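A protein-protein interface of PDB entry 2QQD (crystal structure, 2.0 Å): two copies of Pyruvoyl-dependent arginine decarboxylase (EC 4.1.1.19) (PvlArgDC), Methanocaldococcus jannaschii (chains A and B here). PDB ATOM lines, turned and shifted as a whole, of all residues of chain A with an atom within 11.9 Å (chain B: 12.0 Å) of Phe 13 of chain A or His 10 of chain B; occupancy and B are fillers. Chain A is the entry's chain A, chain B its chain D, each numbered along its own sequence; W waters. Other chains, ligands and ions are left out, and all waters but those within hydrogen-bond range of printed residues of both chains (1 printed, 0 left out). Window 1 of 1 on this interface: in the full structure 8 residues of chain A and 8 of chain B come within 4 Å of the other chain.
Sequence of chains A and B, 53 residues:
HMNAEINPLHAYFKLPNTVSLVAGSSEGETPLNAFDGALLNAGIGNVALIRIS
Water W1 bridges O of His 10 of chain B (2.8 Å) and O of Lys 14 of chain A (2.9 Å).
Ala 11 of chain A touches just one residue of chain B: Phe 13. No residue of chain B comes within 4 Å of Tyr 12 of chain A. Lys 14 of chain A touches just one residue of chain B: Tyr 12 (3.0 Å). No residue of chain B comes within 4 Å of Leu 15 of chain A. Of the printed residues of chain B, Ile 50 of chain A touches Leu 9 and Ile 50. Ile 6 of chain B touches none of the printed residues of chain A. Pro 8 of chain B touches none of the printed residues of chain A. Of the printed residues of chain A, Leu 9 of chain B touches Ile 50. His 10 of chain B touches just one residue of chain A: Phe 13 (3.5 Å). No residue of chain A comes within 4 Å of Ala 11 of chain B. Of the printed residues of chain A, Phe 13 of chain B touches Ala 11. Of the printed residues of chain A, Ile 50 of chain B touches Ile 50 (3.6 Å). The nearest residue of chain A that does not touch His 10 of chain B is Lys 14 of chain A (5.3 Å).
Among the printed residues, pairs that only touch across the chains: Phe 13 of chain A with His 10 of chain B (3.5 Å), Ile 50 of chain A with Leu 9 of chain B (3.6 Å), Ile 50 of chain A with Ile 50 of chain B (3.6 Å) and Ala 11 of chain A with Phe 13 of chain B (3.9 Å).
Hydrophobic or aromatic side chains of chain B that line the printed part of chain A: Leu 9, His 10, Tyr 12, Phe 13 and Ile 50. Hydrophobic or aromatic side chains of chain A that line the printed part of chain B: Ala 11, Phe 13 and Ile 50. Among the printed residues, no Asp or Glu carboxylate lies within 4 Å of a Lys or Arg side-chain nitrogen of the other chain.
NZ of Lys 14 of chain A sits close to OH of Tyr 12 of chain B (3.3 Å).
The side-chain amide oxygen (OD1) of Asn 7 of chain B sits at hydrogen-bond distance from the backbone NH (N) of Leu 9 of chain B (3.0 Å).
Ala 11 of chain A touches Phe 13 of chain B, but with the chains exchanged Phe 13 of chain A does not touch Ala 11 of chain B (6.6 Å). Phe 13 of chain A touches His 10 of chain B, but with the chains exchanged His 10 of chain A does not touch Phe 13 of chain B (7.6 Å). Ile 50 of chain A touches Leu 9 of chain B, but with the chains exchanged Leu 9 of chain A does not touch Ile 50 of chain B (23.6 Å). Ile 50 of chain B touches its own counterpart, Ile 50 of chain A. Of the 5 pairs that touch across the chains among the printed residues, 1 has its exchanged pair printed and touching as well.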
ATOM      1  N   LEU A   9      17.112 -13.104 -15.823  1.00  0.00           N
ATOM      2  CA  LEU A   9      16.705 -12.298 -14.638  1.00  0.00           C
ATOM      3  C   LEU A   9      16.952 -10.812 -14.864  1.00  0.00           C
ATOM      4  O   LEU A   9      16.295  -9.967 -14.265  1.00  0.00           O
ATOM      5  CB  LEU A   9      17.467 -12.765 -13.393  1.00  0.00           C
ATOM      6  CG  LEU A   9      17.135 -14.170 -12.892  1.00  0.00           C
ATOM      7  CD1 LEU A   9      17.960 -14.488 -11.659  1.00  0.00           C
ATOM      8  CD2 LEU A   9      15.651 -14.255 -12.577  1.00  0.00           C
ATOM      9  N   HIS A  10      17.905 -10.499 -15.731  1.00  0.00           N
ATOM     10  CA  HIS A  10      18.223  -9.111 -16.034  1.00  0.00           C
ATOM     11  C   HIS A  10      18.309  -8.942 -17.546  1.00  0.00           C
ATOM     12  O   HIS A  10      19.248  -9.426 -18.181  1.00  0.00           O
ATOM     13  CB  HIS A  10      19.548  -8.715 -15.374  1.00  0.00           C
ATOM     14  CG  HIS A  10      19.912  -7.275 -15.560  1.00  0.00           C
ATOM     15  ND1 HIS A  10      20.666  -6.827 -16.623  1.00  0.00           N
ATOM     16  CD2 HIS A  10      19.608  -6.178 -14.826  1.00  0.00           C
ATOM     17  CE1 HIS A  10      20.811  -5.517 -16.535  1.00  0.00           C
ATOM     18  NE2 HIS A  10      20.179  -5.099 -15.455  1.00  0.00           N
ATOM     19  N   ALA A  11      17.316  -8.266 -18.117  1.00  0.00           N
ATOM     20  CA  ALA A  11      17.269  -8.042 -19.556  1.00  0.00           C
ATOM     21  C   ALA A  11      18.569  -7.424 -20.036  1.00  0.00           C
ATOM     22  O   ALA A  11      19.043  -6.446 -19.468  1.00  0.00           O
ATOM     23  CB  ALA A  11      16.096  -7.137 -19.910  1.00  0.00           C
ATOM     24  N   TYR A  12      19.147  -8.017 -21.074  1.00  0.00           N
ATOM     25  CA  TYR A  12      20.389  -7.525 -21.653  1.00  0.00           C
ATOM     26  C   TYR A  12      20.103  -6.946 -23.034  1.00  0.00           C
ATOM     27  O   TYR A  12      19.440  -7.574 -23.858  1.00  0.00           O
ATOM     28  CB  TYR A  12      21.412  -8.660 -21.761  1.00  0.00           C
ATOM     29  N   PHE A  13      20.600  -5.738 -23.275  1.00  0.00           N
ATOM     30  CA  PHE A  13      20.406  -5.084 -24.556  1.00  0.00           C
ATOM     31  C   PHE A  13      21.109  -5.872 -25.652  1.00  0.00           C
ATOM     32  O   PHE A  13      22.215  -6.382 -25.460  1.00  0.00           O
ATOM     33  CB  PHE A  13      20.955  -3.653 -24.517  1.00  0.00           C
ATOM     34  CG  PHE A  13      21.060  -3.007 -25.872  1.00  0.00           C
ATOM     35  CD1 PHE A  13      19.925  -2.793 -26.647  1.00  0.00           C
ATOM     36  CD2 PHE A  13      22.295  -2.625 -26.379  1.00  0.00           C
ATOM     37  CE1 PHE A  13      20.021  -2.207 -27.910  1.00  0.00           C
ATOM     38  CE2 PHE A  13      22.402  -2.038 -27.641  1.00  0.00           C
ATOM     39  CZ  PHE A  13      21.260  -1.830 -28.407  1.00  0.00           C
ATOM     40  N   LYS A  14      20.456  -5.976 -26.803  1.00  0.00           N
ATOM     41  CA  LYS A  14      21.030  -6.682 -27.931  1.00  0.00           C
ATOM     42  C   LYS A  14      20.425  -6.200 -29.237  1.00  0.00           C
ATOM     43  O   LYS A  14      19.320  -5.669 -29.266  1.00  0.00           O
ATOM     44  CB  LYS A  14      20.811  -8.191 -27.786  1.00  0.00           C
ATOM     45  CG  LYS A  14      19.387  -8.598 -27.492  1.00  0.00           C
ATOM     46  CD  LYS A  14      19.295 -10.102 -27.244  1.00  0.00           C
ATOM     47  CE  LYS A  14      17.921 -10.504 -26.722  1.00  0.00           C
ATOM     48  NZ  LYS A  14      17.855 -11.958 -26.405  1.00  0.00           N
ATOM     49  N   LEU A  15      21.182  -6.369 -30.308  1.00  0.00           N
ATOM     50  CA  LEU A  15      20.731  -6.001 -31.639  1.00  0.00           C
ATOM     51  C   LEU A  15      20.008  -7.229 -32.173  1.00  0.00           C
ATOM     52  O   LEU A  15      20.151  -8.326 -31.624  1.00  0.00           O
ATOM     53  CB  LEU A  15      21.931  -5.694 -32.534  1.00  0.00           C
ATOM     54  CG  LEU A  15      22.539  -4.290 -32.512  1.00  0.00           C
ATOM     55  CD1 LEU A  15      22.661  -3.764 -31.092  1.00  0.00           C
ATOM     56  CD2 LEU A  15      23.893  -4.352 -33.203  1.00  0.00           C
ATOM     57  N   PRO A  16      19.197  -7.062 -33.229  1.00  0.00           N
ATOM     58  CA  PRO A  16      18.496  -8.226 -33.772  1.00  0.00           C
ATOM     59  C   PRO A  16      19.542  -9.272 -34.191  1.00  0.00           C
ATOM     60  O   PRO A  16      20.622  -8.917 -34.667  1.00  0.00           O
ATOM     61  CB  PRO A  16      17.747  -7.643 -34.969  1.00  0.00           C
ATOM     62  CG  PRO A  16      17.479  -6.214 -34.535  1.00  0.00           C
ATOM     63  CD  PRO A  16      18.795  -5.823 -33.922  1.00  0.00           C
ATOM     64  N   ASN A  17      19.228 -10.551 -34.007  1.00  0.00           N
ATOM     65  CA  ASN A  17      20.158 -11.612 -34.373  1.00  0.00           C
ATOM     66  C   ASN A  17      19.565 -12.603 -35.369  1.00  0.00           C
ATOM     67  O   ASN A  17      20.182 -13.624 -35.686  1.00  0.00           O
ATOM     68  CB  ASN A  17      20.643 -12.346 -33.122  1.00  0.00           C
ATOM     69  CG  ASN A  17      19.520 -12.651 -32.168  1.00  0.00           C
ATOM     70  OD1 ASN A  17      18.525 -13.263 -32.546  1.00  0.00           O
ATOM     71  ND2 ASN A  17      19.667 -12.216 -30.916  1.00  0.00           N
ATOM     72  N   ILE A  50       7.923  -1.874 -38.376  1.00  0.00           N
ATOM     73  CA  ILE A  50       8.573  -0.585 -38.180  1.00  0.00           C
ATOM     74  C   ILE A  50       9.542  -0.635 -39.341  1.00  0.00           C
ATOM     75  O   ILE A  50      10.535  -1.368 -39.301  1.00  0.00           O
ATOM     76  CB  ILE A  50       9.398  -0.508 -36.885  1.00  0.00           C
ATOM     77  CG1 ILE A  50       8.485  -0.598 -35.668  1.00  0.00           C
ATOM     78  CG2 ILE A  50      10.180   0.792 -36.852  1.00  0.00           C
ATOM     79  CD1 ILE A  50       9.251  -0.669 -34.352  1.00  0.00           C
ATOM     80  N   ILE A  52      12.503  -0.069 -41.642  1.00  0.00           N
ATOM     81  CA  ILE A  52      13.865   0.408 -41.441  1.00  0.00           C
ATOM     82  C   ILE A  52      14.425   0.792 -42.802  1.00  0.00           C
ATOM     83  O   ILE A  52      14.028   0.233 -43.829  1.00  0.00           O
ATOM     84  CB  ILE A  52      14.775  -0.652 -40.775  1.00  0.00           C
ATOM     85  CG1 ILE A  52      14.836  -1.923 -41.620  1.00  0.00           C
ATOM     86  CG2 ILE A  52      14.258  -0.972 -39.379  1.00  0.00           C
ATOM     87  CD1 ILE A  52      15.736  -3.020 -41.004  1.00  0.00           C
ATOM     88  N   GLU B   5      11.096   5.534 -18.712  1.00  0.00           N
ATOM     89  CA  GLU B   5      11.330   5.715 -20.141  1.00  0.00           C
ATOM     90  C   GLU B   5      11.428   4.382 -20.866  1.00  0.00           C
ATOM     91  O   GLU B   5      11.735   3.356 -20.262  1.00  0.00           O
ATOM     92  CB  GLU B   5      12.626   6.491 -20.373  1.00  0.00           C
ATOM     93  CG  GLU B   5      12.547   7.979 -20.082  1.00  0.00           C
ATOM     94  CD  GLU B   5      13.911   8.651 -20.161  1.00  0.00           C
ATOM     95  OE1 GLU B   5      14.728   8.238 -21.011  1.00  0.00           O
ATOM     96  OE2 GLU B   5      14.164   9.594 -19.379  1.00  0.00           O
ATOM     97  N   ILE B   6      11.162   4.400 -22.166  1.00  0.00           N
ATOM     98  CA  ILE B   6      11.273   3.187 -22.962  1.00  0.00           C
ATOM     99  C   ILE B   6      11.553   3.487 -24.426  1.00  0.00           C
ATOM    100  O   ILE B   6      11.033   4.446 -24.993  1.00  0.00           O
ATOM    101  CB  ILE B   6       9.992   2.314 -22.888  1.00  0.00           C
ATOM    102  CG1 ILE B   6      10.237   0.986 -23.618  1.00  0.00           C
ATOM    103  CG2 ILE B   6       8.809   3.045 -23.525  1.00  0.00           C
ATOM    104  CD1 ILE B   6       9.104  -0.020 -23.490  1.00  0.00           C
ATOM    105  N   ASN B   7      12.411   2.671 -25.022  1.00  0.00           N
ATOM    106  CA  ASN B   7      12.723   2.798 -26.437  1.00  0.00           C
ATOM    107  C   ASN B   7      12.164   1.505 -27.026  1.00  0.00           C
ATOM    108  O   ASN B   7      12.802   0.449 -26.944  1.00  0.00           O
ATOM    109  CB  ASN B   7      14.237   2.868 -26.673  1.00  0.00           C
ATOM    110  CG  ASN B   7      14.583   2.990 -28.147  1.00  0.00           C
ATOM    111  OD1 ASN B   7      13.739   2.739 -29.010  1.00  0.00           O
ATOM    112  ND2 ASN B   7      15.823   3.359 -28.444  1.00  0.00           N
ATOM    113  N   PRO B   8      10.951   1.564 -27.608  1.00  0.00           N
ATOM    114  CA  PRO B   8      10.307   0.388 -28.204  1.00  0.00           C
ATOM    115  C   PRO B   8      11.180  -0.378 -29.208  1.00  0.00           C
ATOM    116  O   PRO B   8      10.960  -1.562 -29.449  1.00  0.00           O
ATOM    117  CB  PRO B   8       9.054   0.973 -28.861  1.00  0.00           C
ATOM    118  CG  PRO B   8       8.744   2.157 -28.006  1.00  0.00           C
ATOM    119  CD  PRO B   8      10.109   2.762 -27.773  1.00  0.00           C
ATOM    120  N   LEU B   9      12.159   0.299 -29.799  1.00  0.00           N
ATOM    121  CA  LEU B   9      13.052  -0.341 -30.764  1.00  0.00           C
ATOM    122  C   LEU B   9      14.023  -1.293 -30.063  1.00  0.00           C
ATOM    123  O   LEU B   9      14.533  -2.234 -30.672  1.00  0.00           O
ATOM    124  CB  LEU B   9      13.847   0.722 -31.530  1.00  0.00           C
ATOM    125  CG  LEU B   9      13.030   1.713 -32.367  1.00  0.00           C
ATOM    126  CD1 LEU B   9      13.938   2.799 -32.924  1.00  0.00           C
ATOM    127  CD2 LEU B   9      12.330   0.970 -33.496  1.00  0.00           C
ATOM    128  N   HIS B  10      14.284  -1.038 -28.784  1.00  0.00           N
ATOM    129  CA  HIS B  10      15.194  -1.876 -28.015  1.00  0.00           C
ATOM    130  C   HIS B  10      14.442  -2.840 -27.099  1.00  0.00           C
ATOM    131  O   HIS B  10      14.819  -4.004 -26.974  1.00  0.00           O
ATOM    132  CB  HIS B  10      16.149  -0.993 -27.211  1.00  0.00           C
ATOM    133  CG  HIS B  10      17.139  -0.258 -28.063  1.00  0.00           C
ATOM    134  ND1 HIS B  10      17.970   0.722 -27.567  1.00  0.00           N
ATOM    135  CD2 HIS B  10      17.445  -0.378 -29.379  1.00  0.00           C
ATOM    136  CE1 HIS B  10      18.746   1.174 -28.537  1.00  0.00           C
ATOM    137  NE2 HIS B  10      18.447   0.523 -29.646  1.00  0.00           N
ATOM    138  N   ALA B  11      13.376  -2.354 -26.469  1.00  0.00           N
ATOM    139  CA  ALA B  11      12.559  -3.188 -25.598  1.00  0.00           C
ATOM    140  C   ALA B  11      11.492  -3.890 -26.454  1.00  0.00           C
ATOM    141  O   ALA B  11      10.295  -3.633 -26.310  1.00  0.00           O
ATOM    142  CB  ALA B  11      11.901  -2.330 -24.525  1.00  0.00           C
ATOM    143  N   TYR B  12      11.944  -4.776 -27.342  1.00  0.00           N
ATOM    144  CA  TYR B  12      11.057  -5.517 -28.239  1.00  0.00           C
ATOM    145  C   TYR B  12      10.133  -6.486 -27.491  1.00  0.00           C
ATOM    146  O   TYR B  12       9.084  -6.876 -28.003  1.00  0.00           O
ATOM    147  CB  TYR B  12      11.899  -6.294 -29.259  1.00  0.00           C
ATOM    148  CG  TYR B  12      12.718  -7.406 -28.646  1.00  0.00           C
ATOM    149  CD1 TYR B  12      12.165  -8.670 -28.446  1.00  0.00           C
ATOM    150  CD2 TYR B  12      14.033  -7.184 -28.218  1.00  0.00           C
ATOM    151  CE1 TYR B  12      12.890  -9.688 -27.838  1.00  0.00           C
ATOM    152  CE2 TYR B  12      14.766  -8.201 -27.601  1.00  0.00           C
ATOM    153  CZ  TYR B  12      14.183  -9.449 -27.416  1.00  0.00           C
ATOM    154  OH  TYR B  12      14.885 -10.469 -26.813  1.00  0.00           O
ATOM    155  N   PHE B  13      10.534  -6.871 -26.279  1.00  0.00           N
ATOM    156  CA  PHE B  13       9.764  -7.806 -25.461  1.00  0.00           C
ATOM    157  C   PHE B  13       8.669  -7.123 -24.637  1.00  0.00           C
ATOM    158  O   PHE B  13       7.860  -7.788 -23.992  1.00  0.00           O
ATOM    159  CB  PHE B  13      10.721  -8.577 -24.540  1.00  0.00           C
ATOM    160  CG  PHE B  13      11.673  -7.688 -23.787  1.00  0.00           C
ATOM    161  CD1 PHE B  13      11.263  -7.024 -22.634  1.00  0.00           C
ATOM    162  CD2 PHE B  13      12.960  -7.471 -24.261  1.00  0.00           C
ATOM    163  CE1 PHE B  13      12.120  -6.156 -21.968  1.00  0.00           C
ATOM    164  CE2 PHE B  13      13.831  -6.600 -23.602  1.00  0.00           C
ATOM    165  CZ  PHE B  13      13.409  -5.942 -22.454  1.00  0.00           C
ATOM    166  N   LYS B  14       8.640  -5.797 -24.649  1.00  0.00           N
ATOM    167  CA  LYS B  14       7.621  -5.067 -23.903  1.00  0.00           C
ATOM    168  C   LYS B  14       6.700  -4.413 -24.926  1.00  0.00           C
ATOM    169  O   LYS B  14       7.044  -3.400 -25.531  1.00  0.00           O
ATOM    170  CB  LYS B  14       8.268  -4.005 -23.002  1.00  0.00           C
ATOM    171  CG  LYS B  14       7.317  -3.372 -21.994  1.00  0.00           C
ATOM    172  CD  LYS B  14       6.647  -4.438 -21.121  1.00  0.00           C
ATOM    173  CE  LYS B  14       6.050  -3.847 -19.846  1.00  0.00           C
ATOM    174  NZ  LYS B  14       4.959  -2.860 -20.084  1.00  0.00           N
ATOM    175  N   LEU B  15       5.533  -5.010 -25.127  1.00  0.00           N
ATOM    176  CA  LEU B  15       4.587  -4.492 -26.106  1.00  0.00           C
ATOM    177  C   LEU B  15       3.605  -3.482 -25.541  1.00  0.00           C
ATOM    178  O   LEU B  15       3.219  -3.560 -24.376  1.00  0.00           O
ATOM    179  CB  LEU B  15       3.810  -5.647 -26.745  1.00  0.00           C
ATOM    180  CG  LEU B  15       4.577  -6.551 -27.718  1.00  0.00           C
ATOM    181  CD1 LEU B  15       5.811  -7.129 -27.047  1.00  0.00           C
ATOM    182  CD2 LEU B  15       3.651  -7.668 -28.191  1.00  0.00           C
ATOM    183  N   PRO B  16       3.193  -2.508 -26.370  1.00  0.00           N
ATOM    184  CA  PRO B  16       2.239  -1.473 -25.956  1.00  0.00           C
ATOM    185  C   PRO B  16       0.951  -2.166 -25.518  1.00  0.00           C
ATOM    186  O   PRO B  16       0.649  -3.266 -25.994  1.00  0.00           O
ATOM    187  CB  PRO B  16       2.034  -0.658 -27.234  1.00  0.00           C
ATOM    188  CG  PRO B  16       3.349  -0.838 -27.972  1.00  0.00           C
ATOM    189  CD  PRO B  16       3.632  -2.303 -27.763  1.00  0.00           C
ATOM    190  N   ILE B  50       7.280   6.885 -34.065  1.00  0.00           N
ATOM    191  CA  ILE B  50       7.892   5.796 -34.814  1.00  0.00           C
ATOM    192  C   ILE B  50       6.704   5.245 -35.599  1.00  0.00           C
ATOM    193  O   ILE B  50       5.803   4.626 -35.030  1.00  0.00           O
ATOM    194  CB  ILE B  50       8.452   4.686 -33.906  1.00  0.00           C
ATOM    195  CG1 ILE B  50       9.596   5.239 -33.052  1.00  0.00           C
ATOM    196  CG2 ILE B  50       8.973   3.523 -34.770  1.00  0.00           C
ATOM    197  CD1 ILE B  50      10.084   4.272 -31.982  1.00  0.00           C
ATOM    198  N   ILE B  52       4.351   2.938 -37.556  1.00  0.00           N
ATOM    199  CA  ILE B  52       4.171   1.510 -37.719  1.00  0.00           C
ATOM    200  C   ILE B  52       3.219   1.269 -38.871  1.00  0.00           C
ATOM    201  O   ILE B  52       2.298   2.050 -39.104  1.00  0.00           O
ATOM    202  CB  ILE B  52       3.636   0.842 -36.444  1.00  0.00           C
ATOM    203  CG1 ILE B  52       2.340   1.515 -35.987  1.00  0.00           C
ATOM    204  CG2 ILE B  52       4.718   0.889 -35.364  1.00  0.00           C
ATOM    205  CD1 ILE B  52       1.664   0.794 -34.834  1.00  0.00           C
HETATM  206  O   HOH W   1      17.285  -5.322 -27.186  1.00  0.00           O
